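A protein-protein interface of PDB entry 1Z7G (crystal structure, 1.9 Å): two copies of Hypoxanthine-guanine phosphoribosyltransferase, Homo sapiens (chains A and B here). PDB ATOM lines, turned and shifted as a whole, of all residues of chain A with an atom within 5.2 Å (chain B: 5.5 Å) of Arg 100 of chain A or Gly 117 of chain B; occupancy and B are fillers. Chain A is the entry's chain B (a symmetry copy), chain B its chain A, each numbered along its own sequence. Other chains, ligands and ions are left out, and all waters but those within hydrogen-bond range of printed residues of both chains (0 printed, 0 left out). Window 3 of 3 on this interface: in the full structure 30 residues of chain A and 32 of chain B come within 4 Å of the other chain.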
ATOM      1  N   LEU A  67     -14.688 -24.427 -14.014  1.00  0.00           N
ATOM      2  CA  LEU A  67     -13.795 -23.815 -14.991  1.00  0.00           C
ATOM      3  C   LEU A  67     -13.750 -22.292 -14.872  1.00  0.00           C
ATOM      4  O   LEU A  67     -14.774 -21.626 -14.986  1.00  0.00           O
ATOM      5  CB  LEU A  67     -14.236 -24.207 -16.402  1.00  0.00           C
ATOM      6  CG  LEU A  67     -14.180 -25.709 -16.705  1.00  0.00           C
ATOM      7  CD1 LEU A  67     -14.897 -26.014 -18.012  1.00  0.00           C
ATOM      8  CD2 LEU A  67     -12.723 -26.156 -16.768  1.00  0.00           C
ATOM      9  N   PHE A  98     -16.798 -31.053 -15.662  1.00  0.00           N
ATOM     10  CA  PHE A  98     -16.352 -29.668 -15.677  1.00  0.00           C
ATOM     11  C   PHE A  98     -17.571 -28.800 -15.933  1.00  0.00           C
ATOM     12  O   PHE A  98     -18.317 -29.031 -16.887  1.00  0.00           O
ATOM     13  CB  PHE A  98     -15.308 -29.446 -16.769  1.00  0.00           C
ATOM     14  CG  PHE A  98     -14.078 -30.283 -16.600  1.00  0.00           C
ATOM     15  CD1 PHE A  98     -14.034 -31.586 -17.093  1.00  0.00           C
ATOM     16  CD2 PHE A  98     -12.976 -29.790 -15.911  1.00  0.00           C
ATOM     17  CE1 PHE A  98     -12.905 -32.387 -16.901  1.00  0.00           C
ATOM     18  CE2 PHE A  98     -11.845 -30.580 -15.710  1.00  0.00           C
ATOM     19  CZ  PHE A  98     -11.811 -31.885 -16.208  1.00  0.00           C
ATOM     20  N   ILE A  99     -17.782 -27.815 -15.067  1.00  0.00           N
ATOM     21  CA  ILE A  99     -18.919 -26.917 -15.199  1.00  0.00           C
ATOM     22  C   ILE A  99     -18.468 -25.468 -15.205  1.00  0.00           C
ATOM     23  O   ILE A  99     -17.335 -25.152 -14.832  1.00  0.00           O
ATOM     24  CB  ILE A  99     -19.912 -27.090 -14.037  1.00  0.00           C
ATOM     25  CG1 ILE A  99     -19.194 -26.844 -12.705  1.00  0.00           C
ATOM     26  CG2 ILE A  99     -20.526 -28.479 -14.082  1.00  0.00           C
ATOM     27  CD1 ILE A  99     -20.127 -26.742 -11.510  1.00  0.00           C
ATOM     28  N   ARG A 100     -19.371 -24.598 -15.634  1.00  0.00           N
ATOM     29  CA  ARG A 100     -19.108 -23.167 -15.689  1.00  0.00           C
ATOM     30  C   ARG A 100     -20.182 -22.425 -14.908  1.00  0.00           C
ATOM     31  O   ARG A 100     -21.321 -22.886 -14.803  1.00  0.00           O
ATOM     32  CB  ARG A 100     -19.108 -22.682 -17.142  1.00  0.00           C
ATOM     33  CG  ARG A 100     -18.005 -23.274 -17.988  1.00  0.00           C
ATOM     34  CD  ARG A 100     -18.091 -22.809 -19.433  1.00  0.00           C
ATOM     35  NE  ARG A 100     -16.981 -23.337 -20.222  1.00  0.00           N
ATOM     36  CZ  ARG A 100     -15.722 -22.932 -20.097  1.00  0.00           C
ATOM     37  NH1 ARG A 100     -15.410 -21.989 -19.216  1.00  0.00           N
ATOM     38  NH2 ARG A 100     -14.770 -23.475 -20.844  1.00  0.00           N
ATOM     39  N   LEU A 101     -19.808 -21.274 -14.358  1.00  0.00           N
ATOM     40  CA  LEU A 101     -20.734 -20.451 -13.592  1.00  0.00           C
ATOM     41  C   LEU A 101     -20.842 -19.074 -14.233  1.00  0.00           C
ATOM     42  O   LEU A 101     -21.819 -18.773 -14.921  1.00  0.00           O
ATOM     43  CB  LEU A 101     -20.245 -20.309 -12.151  1.00  0.00           C
ATOM     44  CG  LEU A 101     -19.921 -21.610 -11.415  1.00  0.00           C
ATOM     45  CD1 LEU A 101     -19.432 -21.286 -10.015  1.00  0.00           C
ATOM     46  CD2 LEU A 101     -21.155 -22.499 -11.362  1.00  0.00           C
ATOM     47  N   LYS A 114     -25.608 -19.337 -13.204  1.00  0.00           N
ATOM     48  CA  LYS A 114     -26.189 -20.549 -13.768  1.00  0.00           C
ATOM     49  C   LYS A 114     -25.102 -21.588 -14.019  1.00  0.00           C
ATOM     50  O   LYS A 114     -24.024 -21.261 -14.510  1.00  0.00           O
ATOM     51  CB  LYS A 114     -26.901 -20.238 -15.086  1.00  0.00           C
ATOM     52  CG  LYS A 114     -27.476 -21.469 -15.780  1.00  0.00           C
ATOM     53  CD  LYS A 114     -28.450 -22.224 -14.866  1.00  0.00           C
ATOM     54  CE  LYS A 114     -29.256 -23.280 -15.631  1.00  0.00           C
ATOM     55  NZ  LYS A 114     -28.399 -24.397 -16.141  1.00  0.00           N
ATOM     56  N   VAL A 115     -25.393 -22.840 -13.681  1.00  0.00           N
ATOM     57  CA  VAL A 115     -24.441 -23.926 -13.871  1.00  0.00           C
ATOM     58  C   VAL A 115     -24.632 -24.567 -15.242  1.00  0.00           C
ATOM     59  O   VAL A 115     -25.756 -24.714 -15.718  1.00  0.00           O
ATOM     60  CB  VAL A 115     -24.607 -25.011 -12.785  1.00  0.00           C
ATOM     61  CG1 VAL A 115     -23.557 -26.095 -12.966  1.00  0.00           C
ATOM     62  CG2 VAL A 115     -24.491 -24.387 -11.405  1.00  0.00           C
ATOM     63  N   ILE A 116     -23.523 -24.947 -15.867  1.00  0.00           N
ATOM     64  CA  ILE A 116     -23.560 -25.572 -17.183  1.00  0.00           C
ATOM     65  C   ILE A 116     -22.931 -26.959 -17.157  1.00  0.00           C
ATOM     66  O   ILE A 116     -21.731 -27.099 -16.924  1.00  0.00           O
ATOM     67  CB  ILE A 116     -22.809 -24.716 -18.219  1.00  0.00           C
ATOM     68  CG1 ILE A 116     -23.466 -23.337 -18.337  1.00  0.00           C
ATOM     69  CG2 ILE A 116     -22.777 -25.429 -19.563  1.00  0.00           C
ATOM     70  CD1 ILE A 116     -24.972 -23.374 -18.590  1.00  0.00           C
ATOM     71  N   ASP B  97      -9.729 -23.510 -23.468  1.00  0.00           N
ATOM     72  CA  ASP B  97     -11.170 -23.551 -23.282  1.00  0.00           C
ATOM     73  C   ASP B  97     -11.720 -24.966 -23.454  1.00  0.00           C
ATOM     74  O   ASP B  97     -11.567 -25.572 -24.508  1.00  0.00           O
ATOM     75  CB  ASP B  97     -11.832 -22.597 -24.281  1.00  0.00           C
ATOM     76  CG  ASP B  97     -13.319 -22.438 -24.047  1.00  0.00           C
ATOM     77  OD1 ASP B  97     -13.744 -22.416 -22.874  1.00  0.00           O
ATOM     78  OD2 ASP B  97     -14.061 -22.315 -25.040  1.00  0.00           O
ATOM     79  N   PHE B  98     -12.334 -25.501 -22.404  1.00  0.00           N
ATOM     80  CA  PHE B  98     -12.927 -26.835 -22.468  1.00  0.00           C
ATOM     81  C   PHE B  98     -14.376 -26.659 -22.892  1.00  0.00           C
ATOM     82  O   PHE B  98     -15.166 -26.075 -22.155  1.00  0.00           O
ATOM     83  CB  PHE B  98     -12.884 -27.528 -21.099  1.00  0.00           C
ATOM     84  CG  PHE B  98     -11.524 -28.048 -20.714  1.00  0.00           C
ATOM     85  CD1 PHE B  98     -11.370 -28.826 -19.575  1.00  0.00           C
ATOM     86  CD2 PHE B  98     -10.401 -27.768 -21.486  1.00  0.00           C
ATOM     87  CE1 PHE B  98     -10.113 -29.307 -19.200  1.00  0.00           C
ATOM     88  CE2 PHE B  98      -9.143 -28.243 -21.122  1.00  0.00           C
ATOM     89  CZ  PHE B  98      -8.998 -29.019 -19.980  1.00  0.00           C
ATOM     90  N   ILE B  99     -14.727 -27.161 -24.071  1.00  0.00           N
ATOM     91  CA  ILE B  99     -16.094 -27.027 -24.562  1.00  0.00           C
ATOM     92  C   ILE B  99     -16.785 -28.366 -24.821  1.00  0.00           C
ATOM     93  O   ILE B  99     -16.139 -29.412 -24.891  1.00  0.00           O
ATOM     94  CB  ILE B  99     -16.143 -26.196 -25.872  1.00  0.00           C
ATOM     95  CG1 ILE B  99     -15.845 -27.084 -27.086  1.00  0.00           C
ATOM     96  CG2 ILE B  99     -15.138 -25.056 -25.805  1.00  0.00           C
ATOM     97  CD1 ILE B  99     -14.463 -27.665 -27.115  1.00  0.00           C
ATOM     98  N   VAL B 115     -22.035 -25.030 -28.919  1.00  0.00           N
ATOM     99  CA  VAL B 115     -20.754 -25.076 -28.228  1.00  0.00           C
ATOM    100  C   VAL B 115     -20.821 -24.324 -26.902  1.00  0.00           C
ATOM    101  O   VAL B 115     -21.273 -23.180 -26.850  1.00  0.00           O
ATOM    102  CB  VAL B 115     -19.632 -24.454 -29.094  1.00  0.00           C
ATOM    103  CG1 VAL B 115     -18.306 -24.503 -28.351  1.00  0.00           C
ATOM    104  CG2 VAL B 115     -19.525 -25.193 -30.419  1.00  0.00           C
ATOM    105  N   ILE B 116     -20.372 -24.978 -25.835  1.00  0.00           N
ATOM    106  CA  ILE B 116     -20.362 -24.372 -24.507  1.00  0.00           C
ATOM    107  C   ILE B 116     -18.937 -23.956 -24.155  1.00  0.00           C
ATOM    108  O   ILE B 116     -18.138 -24.781 -23.714  1.00  0.00           O
ATOM    109  CB  ILE B 116     -20.846 -25.357 -23.416  1.00  0.00           C
ATOM    110  CG1 ILE B 116     -22.283 -25.807 -23.694  1.00  0.00           C
ATOM    111  CG2 ILE B 116     -20.763 -24.695 -22.052  1.00  0.00           C
ATOM    112  CD1 ILE B 116     -22.406 -26.837 -24.798  1.00  0.00           C
ATOM    113  N   GLY B 117     -18.621 -22.679 -24.353  1.00  0.00           N
ATOM    114  CA  GLY B 117     -17.288 -22.195 -24.047  1.00  0.00           C
ATOM    115  C   GLY B 117     -17.296 -21.067 -23.034  1.00  0.00           C
ATOM    116  O   GLY B 117     -18.356 -20.545 -22.685  1.00  0.00           O
ATOM    117  N   GLY B 118     -16.112 -20.693 -22.557  1.00  0.00           N
ATOM    118  CA  GLY B 118     -16.015 -19.621 -21.584  1.00  0.00           C
ATOM    119  C   GLY B 118     -16.191 -18.252 -22.213  1.00  0.00           C
ATOM    120  O   GLY B 118     -16.328 -17.248 -21.509  1.00  0.00           O
ATOM    121  N   ASP B 119     -16.187 -18.209 -23.541  1.00  0.00           N
ATOM    122  CA  ASP B 119     -16.349 -16.954 -24.262  1.00  0.00           C
ATOM    123  C   ASP B 119     -16.820 -17.182 -25.695  1.00  0.00           C
ATOM    124  O   ASP B 119     -16.612 -18.255 -26.266  1.00  0.00           O
ATOM    125  CB  ASP B 119     -15.032 -16.170 -24.257  1.00  0.00           C
ATOM    126  CG  ASP B 119     -13.858 -16.995 -24.744  1.00  0.00           C
ATOM    127  OD1 ASP B 119     -13.568 -18.048 -24.134  1.00  0.00           O
ATOM    128  OD2 ASP B 119     -13.223 -16.586 -25.736  1.00  0.00           O
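The guanidinium group (NH2) of Arg 100 of chain A is in salt-bridge range of the side-chain carboxylate (OD1) of Asp 97 of chain B (2.5 Å).
NH2 of Arg 100 of chain A is in hydrogen-bond range of O of Phe 98 of chain B.
Ile 116 of chain A touches its own counterpart, Ile 116 of chain B.
OD1 of Asp 97 of chain B lies within hydrogen-bond range of N of Gly 118 of chain B (2.9 Å).
O of Ile 99 of chain A is in hydrogen-bond range of N of Leu 67 of chain A, 2.9 Å away.
The backbone NH (N) of Ile 116 of chain A sits at hydrogen-bond distance from the backbone carbonyl oxygen (O) of Arg 100 of chain A (3.2 Å).
Among the printed residues, pairs that only touch across the chains: Leu 67 of chain A with Phe 98 of chain B, Arg 100 of chain A with Ile 116 of chain B, Arg 100 of chain A with Gly 117 of chain B, Arg 100 of chain A with Gly 118 of chain B and Ile 116 of chain A with Ile 116 of chain B.
Hydrophobic or aromatic side chains of chain A within 4 Å of the printed part of chain B: Leu 67 and Ile 116.
Of the 8 printed residues of chain B, 5 touch a printed residue of chain A.
Printed residues of chain B that touch a printed residue of chain A: Asp 97, Phe 98, Ile 116, Gly 117 and Gly 118.
Hydrophobic or aromatic side chains of chain B that line the printed part of chain A: Phe 98 and Ile 116.
Among the printed residues, 7 pairs touch across the chains.
Among the printed residues, Asp or Glu carboxylates within 4 Å of a Lys or Arg side-chain nitrogen of the other chain: Arg 100 of chain A with Asp 97 of chain B (2.5 Å).
Of the printed residues of chain B, Leu 67 of chain A touches Phe 98 (3.98 Å).
Phe 98 of chain A touches none of the printed residues of chain B.
Printed residues of chain A within 4 Å of Phe 98 of chain B: Leu 67 and Arg 100.
Gly 117 of chain B touches just one residue of chain A: Arg 100.
Of the printed residues of chain A, Gly 118 of chain B touches Arg 100 (3.3 Å).
The nearest residue of chain B that does not touch Arg 100 of chain A is Ile 99 of chain B (4.9 Å).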
